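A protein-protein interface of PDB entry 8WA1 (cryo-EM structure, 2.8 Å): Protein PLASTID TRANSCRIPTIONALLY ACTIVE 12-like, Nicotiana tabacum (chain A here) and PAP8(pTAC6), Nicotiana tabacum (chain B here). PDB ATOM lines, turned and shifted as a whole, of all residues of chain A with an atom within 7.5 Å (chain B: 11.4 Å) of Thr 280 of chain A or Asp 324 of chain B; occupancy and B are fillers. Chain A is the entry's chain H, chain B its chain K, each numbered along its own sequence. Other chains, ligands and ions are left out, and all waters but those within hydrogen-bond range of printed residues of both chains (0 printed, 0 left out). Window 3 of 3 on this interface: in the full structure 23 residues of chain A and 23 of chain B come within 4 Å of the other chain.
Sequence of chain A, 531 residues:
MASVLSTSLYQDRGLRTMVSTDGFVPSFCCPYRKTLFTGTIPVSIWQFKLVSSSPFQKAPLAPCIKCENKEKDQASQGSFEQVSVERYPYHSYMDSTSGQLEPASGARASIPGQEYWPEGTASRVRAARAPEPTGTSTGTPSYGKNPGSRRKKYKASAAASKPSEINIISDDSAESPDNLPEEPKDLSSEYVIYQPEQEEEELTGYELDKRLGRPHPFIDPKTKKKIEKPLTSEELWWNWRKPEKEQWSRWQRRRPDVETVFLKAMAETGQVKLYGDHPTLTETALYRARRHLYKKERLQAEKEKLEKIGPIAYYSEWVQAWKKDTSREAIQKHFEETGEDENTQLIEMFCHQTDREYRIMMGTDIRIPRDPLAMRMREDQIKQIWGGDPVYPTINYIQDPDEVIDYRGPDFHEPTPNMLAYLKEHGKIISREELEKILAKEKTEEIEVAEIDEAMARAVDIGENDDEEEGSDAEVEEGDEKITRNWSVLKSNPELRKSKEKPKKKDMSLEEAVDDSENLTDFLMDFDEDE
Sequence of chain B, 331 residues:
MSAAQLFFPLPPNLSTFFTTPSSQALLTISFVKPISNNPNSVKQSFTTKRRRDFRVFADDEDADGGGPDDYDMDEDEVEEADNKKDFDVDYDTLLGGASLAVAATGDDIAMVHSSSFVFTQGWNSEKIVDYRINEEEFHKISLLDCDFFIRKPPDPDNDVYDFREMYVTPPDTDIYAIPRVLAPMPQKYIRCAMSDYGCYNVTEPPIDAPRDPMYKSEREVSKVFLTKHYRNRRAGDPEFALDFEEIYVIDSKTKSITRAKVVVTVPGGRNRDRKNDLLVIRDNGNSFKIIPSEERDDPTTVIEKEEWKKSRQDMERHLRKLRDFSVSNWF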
ATOM      1  N   PHE A 218     -22.693 -12.938 -11.222  1.00  0.00           N
ATOM      2  CA  PHE A 218     -21.409 -13.213 -10.587  1.00  0.00           C
ATOM      3  C   PHE A 218     -20.676 -14.355 -11.281  1.00  0.00           C
ATOM      4  O   PHE A 218     -19.446 -14.327 -11.402  1.00  0.00           O
ATOM      5  CB  PHE A 218     -21.609 -13.533  -9.106  1.00  0.00           C
ATOM      6  CG  PHE A 218     -21.821 -12.322  -8.244  1.00  0.00           C
ATOM      7  CD1 PHE A 218     -20.744 -11.563  -7.819  1.00  0.00           C
ATOM      8  CD2 PHE A 218     -23.093 -11.949  -7.846  1.00  0.00           C
ATOM      9  CE1 PHE A 218     -20.932 -10.453  -7.022  1.00  0.00           C
ATOM     10  CE2 PHE A 218     -23.288 -10.840  -7.048  1.00  0.00           C
ATOM     11  CZ  PHE A 218     -22.206 -10.091  -6.634  1.00  0.00           C
ATOM     12  N   ARG A 254     -39.410 -16.251   3.874  1.00  0.00           N
ATOM     13  CA  ARG A 254     -38.301 -15.311   3.811  1.00  0.00           C
ATOM     14  C   ARG A 254     -38.675 -14.040   4.562  1.00  0.00           C
ATOM     15  O   ARG A 254     -39.748 -13.472   4.335  1.00  0.00           O
ATOM     16  CB  ARG A 254     -37.942 -14.995   2.358  1.00  0.00           C
ATOM     17  CG  ARG A 254     -36.650 -14.219   2.178  1.00  0.00           C
ATOM     18  CD  ARG A 254     -36.136 -14.355   0.752  1.00  0.00           C
ATOM     19  NE  ARG A 254     -34.941 -13.551   0.516  1.00  0.00           N
ATOM     20  CZ  ARG A 254     -34.952 -12.350  -0.051  1.00  0.00           C
ATOM     21  NH1 ARG A 254     -36.096 -11.811  -0.444  1.00  0.00           N
ATOM     22  NH2 ARG A 254     -33.817 -11.689  -0.229  1.00  0.00           N
ATOM     23  N   GLU A 259     -34.677  -3.781   2.223  1.00  0.00           N
ATOM     24  CA  GLU A 259     -33.771  -3.990   1.099  1.00  0.00           C
ATOM     25  C   GLU A 259     -34.469  -4.704  -0.052  1.00  0.00           C
ATOM     26  O   GLU A 259     -34.307  -4.322  -1.216  1.00  0.00           O
ATOM     27  CB  GLU A 259     -32.549  -4.779   1.563  1.00  0.00           C
ATOM     28  CG  GLU A 259     -31.869  -4.182   2.785  1.00  0.00           C
ATOM     29  CD  GLU A 259     -30.789  -5.081   3.352  1.00  0.00           C
ATOM     30  OE1 GLU A 259     -30.606  -6.199   2.827  1.00  0.00           O
ATOM     31  OE2 GLU A 259     -30.125  -4.669   4.325  1.00  0.00           O
ATOM     32  N   THR A 260     -35.255  -5.740   0.254  1.00  0.00           N
ATOM     33  CA  THR A 260     -35.961  -6.469  -0.796  1.00  0.00           C
ATOM     34  C   THR A 260     -36.987  -5.580  -1.489  1.00  0.00           C
ATOM     35  O   THR A 260     -37.116  -5.608  -2.719  1.00  0.00           O
ATOM     36  CB  THR A 260     -36.635  -7.709  -0.211  1.00  0.00           C
ATOM     37  OG1 THR A 260     -35.657  -8.518   0.453  1.00  0.00           O
ATOM     38  CG2 THR A 260     -37.297  -8.526  -1.311  1.00  0.00           C
ATOM     39  N   LEU A 263     -35.147  -3.128  -3.714  1.00  0.00           N
ATOM     40  CA  LEU A 263     -34.613  -3.807  -4.889  1.00  0.00           C
ATOM     41  C   LEU A 263     -35.714  -4.119  -5.892  1.00  0.00           C
ATOM     42  O   LEU A 263     -35.506  -4.011  -7.104  1.00  0.00           O
ATOM     43  CB  LEU A 263     -33.884  -5.084  -4.477  1.00  0.00           C
ATOM     44  CG  LEU A 263     -32.462  -4.901  -3.946  1.00  0.00           C
ATOM     45  CD1 LEU A 263     -31.838  -6.244  -3.610  1.00  0.00           C
ATOM     46  CD2 LEU A 263     -31.616  -4.154  -4.963  1.00  0.00           C
ATOM     47  N   LEU A 274     -31.528  -7.681 -11.811  1.00  0.00           N
ATOM     48  CA  LEU A 274     -31.342  -8.768 -10.865  1.00  0.00           C
ATOM     49  C   LEU A 274     -31.465 -10.108 -11.578  1.00  0.00           C
ATOM     50  O   LEU A 274     -32.168 -10.233 -12.585  1.00  0.00           O
ATOM     51  CB  LEU A 274     -32.364  -8.695  -9.725  1.00  0.00           C
ATOM     52  CG  LEU A 274     -32.413  -7.370  -8.961  1.00  0.00           C
ATOM     53  CD1 LEU A 274     -33.449  -7.427  -7.853  1.00  0.00           C
ATOM     54  CD2 LEU A 274     -31.044  -7.024  -8.401  1.00  0.00           C
ATOM     55  N   TYR A 275     -30.772 -11.109 -11.043  1.00  0.00           N
ATOM     56  CA  TYR A 275     -30.821 -12.455 -11.595  1.00  0.00           C
ATOM     57  C   TYR A 275     -32.140 -13.106 -11.202  1.00  0.00           C
ATOM     58  O   TYR A 275     -32.232 -13.754 -10.153  1.00  0.00           O
ATOM     59  CB  TYR A 275     -29.637 -13.278 -11.096  1.00  0.00           C
ATOM     60  CG  TYR A 275     -29.377 -14.535 -11.893  1.00  0.00           C
ATOM     61  CD1 TYR A 275     -30.035 -15.720 -11.594  1.00  0.00           C
ATOM     62  CD2 TYR A 275     -28.474 -14.535 -12.946  1.00  0.00           C
ATOM     63  CE1 TYR A 275     -29.800 -16.869 -12.324  1.00  0.00           C
ATOM     64  CE2 TYR A 275     -28.231 -15.680 -13.680  1.00  0.00           C
ATOM     65  CZ  TYR A 275     -28.896 -16.844 -13.365  1.00  0.00           C
ATOM     66  OH  TYR A 275     -28.658 -17.987 -14.093  1.00  0.00           O
ATOM     67  N   ASP A 277     -36.643 -12.740 -10.992  1.00  0.00           N
ATOM     68  CA  ASP A 277     -37.721 -11.816 -10.670  1.00  0.00           C
ATOM     69  C   ASP A 277     -37.806 -11.462  -9.192  1.00  0.00           C
ATOM     70  O   ASP A 277     -38.529 -10.522  -8.842  1.00  0.00           O
ATOM     71  CB  ASP A 277     -39.068 -12.395 -11.127  1.00  0.00           C
ATOM     72  CG  ASP A 277     -39.321 -13.787 -10.580  1.00  0.00           C
ATOM     73  OD1 ASP A 277     -39.590 -13.913  -9.366  1.00  0.00           O
ATOM     74  OD2 ASP A 277     -39.250 -14.758 -11.363  1.00  0.00           O
ATOM     75  N   HIS A 278     -37.097 -12.176  -8.320  1.00  0.00           N
ATOM     76  CA  HIS A 278     -37.139 -11.929  -6.891  1.00  0.00           C
ATOM     77  C   HIS A 278     -35.729 -11.706  -6.362  1.00  0.00           C
ATOM     78  O   HIS A 278     -34.830 -12.508  -6.654  1.00  0.00           O
ATOM     79  CB  HIS A 278     -37.797 -13.105  -6.149  1.00  0.00           C
ATOM     80  CG  HIS A 278     -38.085 -12.826  -4.707  1.00  0.00           C
ATOM     81  ND1 HIS A 278     -38.887 -11.783  -4.297  1.00  0.00           N
ATOM     82  CD2 HIS A 278     -37.681 -13.457  -3.579  1.00  0.00           C
ATOM     83  CE1 HIS A 278     -38.963 -11.781  -2.977  1.00  0.00           C
ATOM     84  NE2 HIS A 278     -38.240 -12.786  -2.518  1.00  0.00           N
ATOM     85  N   PRO A 279     -35.489 -10.641  -5.597  1.00  0.00           N
ATOM     86  CA  PRO A 279     -34.135 -10.391  -5.088  1.00  0.00           C
ATOM     87  C   PRO A 279     -33.698 -11.473  -4.113  1.00  0.00           C
ATOM     88  O   PRO A 279     -34.475 -11.929  -3.271  1.00  0.00           O
ATOM     89  CB  PRO A 279     -34.261  -9.028  -4.394  1.00  0.00           C
ATOM     90  CG  PRO A 279     -35.516  -8.421  -4.942  1.00  0.00           C
ATOM     91  CD  PRO A 279     -36.427  -9.570  -5.226  1.00  0.00           C
ATOM     92  N   THR A 280     -32.440 -11.882  -4.234  1.00  0.00           N
ATOM     93  CA  THR A 280     -31.850 -12.869  -3.345  1.00  0.00           C
ATOM     94  C   THR A 280     -31.059 -12.180  -2.239  1.00  0.00           C
ATOM     95  O   THR A 280     -30.828 -10.968  -2.268  1.00  0.00           O
ATOM     96  CB  THR A 280     -30.949 -13.835  -4.117  1.00  0.00           C
ATOM     97  OG1 THR A 280     -30.367 -14.776  -3.207  1.00  0.00           O
ATOM     98  CG2 THR A 280     -29.843 -13.081  -4.831  1.00  0.00           C
ATOM     99  N   LEU A 281     -30.642 -12.979  -1.254  1.00  0.00           N
ATOM    100  CA  LEU A 281     -29.996 -12.425  -0.067  1.00  0.00           C
ATOM    101  C   LEU A 281     -28.670 -11.754  -0.407  1.00  0.00           C
ATOM    102  O   LEU A 281     -28.311 -10.733   0.193  1.00  0.00           O
ATOM    103  CB  LEU A 281     -29.799 -13.522   0.977  1.00  0.00           C
ATOM    104  CG  LEU A 281     -31.102 -14.097   1.539  1.00  0.00           C
ATOM    105  CD1 LEU A 281     -30.824 -15.238   2.497  1.00  0.00           C
ATOM    106  CD2 LEU A 281     -31.910 -13.009   2.226  1.00  0.00           C
ATOM    107  N   THR A 282     -27.925 -12.312  -1.364  1.00  0.00           N
ATOM    108  CA  THR A 282     -26.683 -11.673  -1.788  1.00  0.00           C
ATOM    109  C   THR A 282     -26.955 -10.305  -2.400  1.00  0.00           C
ATOM    110  O   THR A 282     -26.229  -9.338  -2.135  1.00  0.00           O
ATOM    111  CB  THR A 282     -25.944 -12.566  -2.784  1.00  0.00           C
ATOM    112  OG1 THR A 282     -26.633 -12.553  -4.040  1.00  0.00           O
ATOM    113  CG2 THR A 282     -25.882 -13.995  -2.269  1.00  0.00           C
ATOM    114  N   GLU A 283     -28.008 -10.202  -3.214  1.00  0.00           N
ATOM    115  CA  GLU A 283     -28.365  -8.913  -3.798  1.00  0.00           C
ATOM    116  C   GLU A 283     -28.843  -7.937  -2.732  1.00  0.00           C
ATOM    117  O   GLU A 283     -28.562  -6.737  -2.814  1.00  0.00           O
ATOM    118  CB  GLU A 283     -29.427  -9.105  -4.879  1.00  0.00           C
ATOM    119  CG  GLU A 283     -28.926  -9.851  -6.105  1.00  0.00           C
ATOM    120  CD  GLU A 283     -30.038 -10.190  -7.074  1.00  0.00           C
ATOM    121  OE1 GLU A 283     -31.214  -9.932  -6.745  1.00  0.00           O
ATOM    122  OE2 GLU A 283     -29.738 -10.716  -8.167  1.00  0.00           O
ATOM    123  N   THR A 284     -29.559  -8.429  -1.716  1.00  0.00           N
ATOM    124  CA  THR A 284     -29.985  -7.546  -0.635  1.00  0.00           C
ATOM    125  C   THR A 284     -28.790  -7.025   0.153  1.00  0.00           C
ATOM    126  O   THR A 284     -28.766  -5.856   0.549  1.00  0.00           O
ATOM    127  CB  THR A 284     -30.965  -8.264   0.293  1.00  0.00           C
ATOM    128  OG1 THR A 284     -30.326  -9.402   0.884  1.00  0.00           O
ATOM    129  CG2 THR A 284     -32.199  -8.714  -0.475  1.00  0.00           C
ATOM    130  N   ALA A 285     -27.782  -7.872   0.377  1.00  0.00           N
ATOM    131  CA  ALA A 285     -26.574  -7.411   1.056  1.00  0.00           C
ATOM    132  C   ALA A 285     -25.815  -6.398   0.204  1.00  0.00           C
ATOM    133  O   ALA A 285     -25.326  -5.381   0.714  1.00  0.00           O
ATOM    134  CB  ALA A 285     -25.680  -8.600   1.406  1.00  0.00           C
ATOM    135  N   LEU A 286     -25.713  -6.657  -1.103  1.00  0.00           N
ATOM    136  CA  LEU A 286     -25.052  -5.709  -1.995  1.00  0.00           C
ATOM    137  C   LEU A 286     -25.776  -4.367  -2.003  1.00  0.00           C
ATOM    138  O   LEU A 286     -25.140  -3.306  -2.038  1.00  0.00           O
ATOM    139  CB  LEU A 286     -24.978  -6.290  -3.406  1.00  0.00           C
ATOM    140  CG  LEU A 286     -24.053  -5.587  -4.399  1.00  0.00           C
ATOM    141  CD1 LEU A 286     -22.606  -5.698  -3.947  1.00  0.00           C
ATOM    142  CD2 LEU A 286     -24.229  -6.167  -5.793  1.00  0.00           C
ATOM    143  N   MET B 315     -15.276  -7.778  -1.747  1.00  0.00           N
ATOM    144  CA  MET B 315     -16.717  -7.979  -1.653  1.00  0.00           C
ATOM    145  C   MET B 315     -17.131  -9.288  -2.312  1.00  0.00           C
ATOM    146  O   MET B 315     -17.993 -10.006  -1.791  1.00  0.00           O
ATOM    147  CB  MET B 315     -17.454  -6.800  -2.287  1.00  0.00           C
ATOM    148  CG  MET B 315     -18.944  -6.770  -1.994  1.00  0.00           C
ATOM    149  SD  MET B 315     -19.296  -6.583  -0.236  1.00  0.00           S
ATOM    150  CE  MET B 315     -21.085  -6.515  -0.251  1.00  0.00           C
ATOM    151  N   GLU B 316     -16.528  -9.617  -3.457  1.00  0.00           N
ATOM    152  CA  GLU B 316     -16.811 -10.906  -4.079  1.00  0.00           C
ATOM    153  C   GLU B 316     -16.342 -12.052  -3.191  1.00  0.00           C
ATOM    154  O   GLU B 316     -17.044 -13.061  -3.043  1.00  0.00           O
ATOM    155  CB  GLU B 316     -16.154 -10.982  -5.457  1.00  0.00           C
ATOM    156  CG  GLU B 316     -16.489 -12.246  -6.231  1.00  0.00           C
ATOM    157  CD  GLU B 316     -15.981 -12.208  -7.659  1.00  0.00           C
ATOM    158  OE1 GLU B 316     -15.317 -11.218  -8.029  1.00  0.00           O
ATOM    159  OE2 GLU B 316     -16.251 -13.168  -8.411  1.00  0.00           O
ATOM    160  N   HIS B 318     -16.179 -12.026   0.027  1.00  0.00           N
ATOM    161  CA  HIS B 318     -17.090 -12.120   1.163  1.00  0.00           C
ATOM    162  C   HIS B 318     -18.416 -12.753   0.760  1.00  0.00           C
ATOM    163  O   HIS B 318     -18.952 -13.604   1.480  1.00  0.00           O
ATOM    164  CB  HIS B 318     -17.318 -10.732   1.766  1.00  0.00           C
ATOM    165  CG  HIS B 318     -18.355 -10.704   2.844  1.00  0.00           C
ATOM    166  ND1 HIS B 318     -18.202 -11.371   4.041  1.00  0.00           N
ATOM    167  CD2 HIS B 318     -19.561 -10.092   2.906  1.00  0.00           C
ATOM    168  CE1 HIS B 318     -19.268 -11.169   4.794  1.00  0.00           C
ATOM    169  NE2 HIS B 318     -20.108 -10.397   4.129  1.00  0.00           N
ATOM    170  N   LEU B 319     -18.960 -12.355  -0.390  1.00  0.00           N
ATOM    171  CA  LEU B 319     -20.264 -12.845  -0.816  1.00  0.00           C
ATOM    172  C   LEU B 319     -20.215 -14.240  -1.423  1.00  0.00           C
ATOM    173  O   LEU B 319     -21.276 -14.843  -1.621  1.00  0.00           O
ATOM    174  CB  LEU B 319     -20.888 -11.876  -1.823  1.00  0.00           C
ATOM    175  CG  LEU B 319     -21.221 -10.477  -1.303  1.00  0.00           C
ATOM    176  CD1 LEU B 319     -21.860  -9.638  -2.398  1.00  0.00           C
ATOM    177  CD2 LEU B 319     -22.130 -10.560  -0.088  1.00  0.00           C
ATOM    178  N   ARG B 320     -19.025 -14.766  -1.727  1.00  0.00           N
ATOM    179  CA  ARG B 320     -18.947 -16.100  -2.316  1.00  0.00           C
ATOM    180  C   ARG B 320     -19.462 -17.172  -1.359  1.00  0.00           C
ATOM    181  O   ARG B 320     -20.059 -18.163  -1.794  1.00  0.00           O
ATOM    182  CB  ARG B 320     -17.508 -16.402  -2.737  1.00  0.00           C
ATOM    183  CG  ARG B 320     -17.352 -17.695  -3.517  1.00  0.00           C
ATOM    184  CD  ARG B 320     -15.933 -17.858  -4.036  1.00  0.00           C
ATOM    185  NE  ARG B 320     -15.537 -16.746  -4.894  1.00  0.00           N
ATOM    186  CZ  ARG B 320     -15.776 -16.687  -6.200  1.00  0.00           C
ATOM    187  NH1 ARG B 320     -16.412 -17.681  -6.805  1.00  0.00           N
ATOM    188  NH2 ARG B 320     -15.380 -15.634  -6.901  1.00  0.00           N
ATOM    189  N   LYS B 321     -19.242 -16.994  -0.054  1.00  0.00           N
ATOM    190  CA  LYS B 321     -19.618 -18.028   0.904  1.00  0.00           C
ATOM    191  C   LYS B 321     -21.127 -18.170   1.060  1.00  0.00           C
ATOM    192  O   LYS B 321     -21.586 -19.170   1.623  1.00  0.00           O
ATOM    193  CB  LYS B 321     -18.985 -17.745   2.268  1.00  0.00           C
ATOM    194  CG  LYS B 321     -19.460 -16.462   2.924  1.00  0.00           C
ATOM    195  CD  LYS B 321     -19.059 -16.418   4.389  1.00  0.00           C
ATOM    196  CE  LYS B 321     -17.562 -16.608   4.559  1.00  0.00           C
ATOM    197  NZ  LYS B 321     -17.166 -16.619   5.994  1.00  0.00           N
ATOM    198  N   LEU B 322     -21.907 -17.201   0.584  1.00  0.00           N
ATOM    199  CA  LEU B 322     -23.357 -17.294   0.689  1.00  0.00           C
ATOM    200  C   LEU B 322     -23.887 -18.361  -0.261  1.00  0.00           C
ATOM    201  O   LEU B 322     -23.401 -18.504  -1.387  1.00  0.00           O
ATOM    202  CB  LEU B 322     -24.000 -15.942   0.389  1.00  0.00           C
ATOM    203  CG  LEU B 322     -23.655 -14.821   1.372  1.00  0.00           C
ATOM    204  CD1 LEU B 322     -24.396 -13.540   1.023  1.00  0.00           C
ATOM    205  CD2 LEU B 322     -23.965 -15.248   2.799  1.00  0.00           C
ATOM    206  N   ARG B 323     -24.888 -19.117   0.199  1.00  0.00           N
ATOM    207  CA  ARG B 323     -25.400 -20.246  -0.570  1.00  0.00           C
ATOM    208  C   ARG B 323     -26.160 -19.821  -1.820  1.00  0.00           C
ATOM    209  O   ARG B 323     -26.497 -20.683  -2.638  1.00  0.00           O
ATOM    210  CB  ARG B 323     -26.299 -21.114   0.314  1.00  0.00           C
ATOM    211  CG  ARG B 323     -25.741 -21.349   1.709  1.00  0.00           C
ATOM    212  CD  ARG B 323     -26.257 -22.642   2.322  1.00  0.00           C
ATOM    213  NE  ARG B 323     -27.715 -22.722   2.318  1.00  0.00           N
ATOM    214  CZ  ARG B 323     -28.406 -23.704   2.889  1.00  0.00           C
ATOM    215  NH1 ARG B 323     -27.772 -24.686   3.513  1.00  0.00           N
ATOM    216  NH2 ARG B 323     -29.731 -23.702   2.838  1.00  0.00           N
ATOM    217  N   ASP B 324     -26.438 -18.530  -1.989  1.00  0.00           N
ATOM    218  CA  ASP B 324     -27.116 -18.024  -3.176  1.00  0.00           C
ATOM    219  C   ASP B 324     -26.185 -17.230  -4.084  1.00  0.00           C
ATOM    220  O   ASP B 324     -26.663 -16.485  -4.945  1.00  0.00           O
ATOM    221  CB  ASP B 324     -28.315 -17.164  -2.774  1.00  0.00           C
ATOM    222  CG  ASP B 324     -29.404 -17.966  -2.093  1.00  0.00           C
ATOM    223  OD1 ASP B 324     -29.223 -19.189  -1.916  1.00  0.00           O
ATOM    224  OD2 ASP B 324     -30.444 -17.373  -1.735  1.00  0.00           O
ATOM    225  N   PHE B 325     -24.869 -17.370  -3.907  1.00  0.00           N
ATOM    226  CA  PHE B 325     -23.925 -16.626  -4.734  1.00  0.00           C
ATOM    227  C   PHE B 325     -24.010 -17.047  -6.195  1.00  0.00           C
ATOM    228  O   PHE B 325     -23.761 -16.239  -7.097  1.00  0.00           O
ATOM    229  CB  PHE B 325     -22.504 -16.815  -4.201  1.00  0.00           C
ATOM    230  CG  PHE B 325     -21.456 -16.082  -4.989  1.00  0.00           C
ATOM    231  CD1 PHE B 325     -21.251 -14.726  -4.799  1.00  0.00           C
ATOM    232  CD2 PHE B 325     -20.668 -16.751  -5.911  1.00  0.00           C
ATOM    233  CE1 PHE B 325     -20.285 -14.051  -5.517  1.00  0.00           C
ATOM    234  CE2 PHE B 325     -19.701 -16.079  -6.633  1.00  0.00           C
ATOM    235  CZ  PHE B 325     -19.510 -14.727  -6.436  1.00  0.00           C
ATOM    236  N   SER B 326     -24.353 -18.313  -6.450  1.00  0.00           N
ATOM    237  CA  SER B 326     -24.422 -18.802  -7.822  1.00  0.00           C
ATOM    238  C   SER B 326     -25.499 -18.071  -8.614  1.00  0.00           C
ATOM    239  O   SER B 326     -25.220 -17.472  -9.660  1.00  0.00           O
ATOM    240  CB  SER B 326     -24.676 -20.310  -7.828  1.00  0.00           C
ATOM    241  OG  SER B 326     -23.599 -21.012  -7.233  1.00  0.00           O
ATOM    242  N   VAL B 327     -26.737 -18.110  -8.133  1.00  0.00           N
ATOM    243  CA  VAL B 327     -27.846 -17.400  -8.796  1.00  0.00           C
ATOM    244  C   VAL B 327     -27.897 -16.013  -8.164  1.00  0.00           C
ATOM    245  O   VAL B 327     -28.627 -15.743  -7.207  1.00  0.00           O
ATOM    246  CB  VAL B 327     -29.170 -18.162  -8.685  1.00  0.00           C
ATOM    247  CG1 VAL B 327     -29.271 -19.202  -9.787  1.00  0.00           C
ATOM    248  CG2 VAL B 327     -29.284 -18.832  -7.325  1.00  0.00           C
ATOM    249  N   SER B 328     -27.095 -15.107  -8.718  1.00  0.00           N
ATOM    250  CA  SER B 328     -27.014 -13.741  -8.221  1.00  0.00           C
ATOM    251  C   SER B 328     -26.556 -12.832  -9.352  1.00  0.00           C
ATOM    252  O   SER B 328     -26.173 -13.291 -10.431  1.00  0.00           O
ATOM    253  CB  SER B 328     -26.068 -13.637  -7.020  1.00  0.00           C
ATOM    254  OG  SER B 328     -26.555 -14.380  -5.916  1.00  0.00           O
ATOM    255  N   ASN B 329     -26.599 -11.528  -9.090  1.00  0.00           N
ATOM    256  CA  ASN B 329     -26.210 -10.534 -10.081  1.00  0.00           C
ATOM    257  C   ASN B 329     -25.601  -9.340  -9.364  1.00  0.00           C
ATOM    258  O   ASN B 329     -26.218  -8.784  -8.451  1.00  0.00           O
ATOM    259  CB  ASN B 329     -27.415 -10.100 -10.925  1.00  0.00           C
ATOM    260  CG  ASN B 329     -27.014  -9.331 -12.169  1.00  0.00           C
ATOM    261  OD1 ASN B 329     -26.169  -8.438 -12.121  1.00  0.00           O
ATOM    262  ND2 ASN B 329     -27.622  -9.679 -13.297  1.00  0.00           N
ATOM    263  N   TRP B 330     -24.396  -8.954  -9.775  1.00  0.00           N
ATOM    264  CA  TRP B 330     -23.739  -7.790  -9.200  1.00  0.00           C
ATOM    265  C   TRP B 330     -24.249  -6.526  -9.879  1.00  0.00           C
ATOM    266  O   TRP B 330     -24.029  -6.324 -11.076  1.00  0.00           O
ATOM    267  CB  TRP B 330     -22.222  -7.895  -9.351  1.00  0.00           C
ATOM    268  CG  TRP B 330     -21.466  -6.882  -8.539  1.00  0.00           C
ATOM    269  CD1 TRP B 330     -20.958  -7.054  -7.284  1.00  0.00           C
ATOM    270  CD2 TRP B 330     -21.137  -5.543  -8.924  1.00  0.00           C
ATOM    271  NE1 TRP B 330     -20.332  -5.906  -6.864  1.00  0.00           N
ATOM    272  CE2 TRP B 330     -20.428  -4.962  -7.854  1.00  0.00           C
ATOM    273  CE3 TRP B 330     -21.371  -4.778 -10.070  1.00  0.00           C
ATOM    274  CZ2 TRP B 330     -19.953  -3.654  -7.894  1.00  0.00           C
ATOM    275  CZ3 TRP B 330     -20.900  -3.480 -10.108  1.00  0.00           C
ATOM    276  CH2 TRP B 330     -20.198  -2.931  -9.028  1.00  0.00           C
ATOM    277  N   PHE B 331     -24.923  -5.676  -9.113  1.00  0.00           N
ATOM    278  CA  PHE B 331     -25.493  -4.449  -9.654  1.00  0.00           C
ATOM    279  C   PHE B 331     -24.847  -3.221  -9.022  1.00  0.00           C
ATOM    280  O   PHE B 331     -24.897  -2.124  -9.576  1.00  0.00           O
ATOM    281  CB  PHE B 331     -27.009  -4.422  -9.438  1.00  0.00           C
ATOM    282  CG  PHE B 331     -27.421  -4.623  -8.008  1.00  0.00           C
ATOM    283  CD1 PHE B 331     -27.649  -5.895  -7.511  1.00  0.00           C
ATOM    284  CD2 PHE B 331     -27.583  -3.540  -7.160  1.00  0.00           C
ATOM    285  CE1 PHE B 331     -28.027  -6.082  -6.198  1.00  0.00           C
ATOM    286  CE2 PHE B 331     -27.961  -3.722  -5.846  1.00  0.00           C
ATOM    287  CZ  PHE B 331     -28.183  -4.995  -5.364  1.00  0.00           C
ATOM    288  OXT PHE B 331     -24.261  -3.300  -7.943  1.00  0.00           O
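His 278 of chain A touches none of the printed residues of chain B. No residue of chain B comes within 4 Å of Pro 279 of chain A. Of the printed residues of chain B, Thr 280 of chain A touches Asp 324, Val 327 and Ser 328. No residue of chain B comes within 4 Å of Leu 281 of chain A. Of the printed residues of chain B, Leu 286 of chain A touches Trp 330 (3.7 Å) and Phe 331 (3.4 Å). Of chain A, only Thr 280 (3.0 Å) and Thr 282 (3.7 Å) come within 4 Å of Asp 324 of chain B. Printed residues of chain A within 4 Å of Asn 329 of chain B: Phe 218 (3.6 Å), Tyr 275 (3.5 Å) and Glu 283 (3.4 Å). The nearest residue of chain A that does not touch Asp 324 of chain B is Leu 281 of chain A (4.4 Å). The nearest printed residue of chain A that does not touch Val 327 of chain B is Thr 282 of chain A (4.9 Å).
OE2 of Glu 283 of chain A sits at hydrogen-bond distance from N of Tyr 275 of chain A. The side-chain carboxylate (OE1) of Glu 283 of chain A lies within hydrogen-bond range of the backbone NH (N) of Thr 280 of chain A (3.4 Å).
OG1 of Thr 280 of chain A sits at hydrogen-bond distance from OD2 of Asp 324 of chain B (3.0 Å). The side-chain hydroxyl of Ser 328 of chain B lies within hydrogen-bond range of the side-chain hydroxyl of Thr 282 of chain A (2.6 Å). The side-chain carboxylate of Glu 283 of chain A sits at hydrogen-bond distance from the backbone NH of Asn 329 of chain B.
Of the 17 printed residues of chain A, 8 touch a printed residue of chain B. Along chain A the printed residues that touch a printed residue of chain B span positions 218 to 286. Of the 16 printed residues of chain B, 8 touch a printed residue of chain A. Hydrophobic or aromatic side chains of chain B that line the printed part of chain A: Leu 322, Phe 325, Val 327, Trp 330 and Phe 331. Along chain B the printed residues that touch a printed residue of chain A span positions 322 to 331.
Among the printed residues, merely in contact across the chains: Phe 218 of chain A with Phe 325 of chain B (3.4 Å), Phe 218 of chain A with Ser 328 of chain B (3.5 Å), Phe 218 of chain A with Asn 329 of chain B (3.6 Å), Phe 218 of chain A with Trp 330 of chain B (3.3 Å), Leu 263 of chain A with Phe 331 of chain B (3.6 Å), Leu 274 of chain A with Phe 331 of chain B (3.7 Å), Tyr 275 of chain A with Val 327 of chain B (3.5 Å), Tyr 275 of chain A with Ser 328 of chain B (3.5 Å), Tyr 275 of chain A with Asn 329 of chain B (3.5 Å), Thr 280 of chain A with Val 327 of chain B (3.8 Å), Thr 280 of chain A with Ser 328 of chain B (3.7 Å), Thr 282 of chain A with Leu 322 of chain B (3.6 Å), Thr 282 of chain A with Asp 324 of chain B (3.7 Å), Thr 282 of chain A with Phe 325 of chain B (3.9 Å), Glu 283 of chain A with Phe 331 of chain B (3.1 Å), Leu 286 of chain A with Trp 330 of chain B (3.7 Å) and Leu 286 of chain A with Phe 331 of chain B (3.4 Å).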
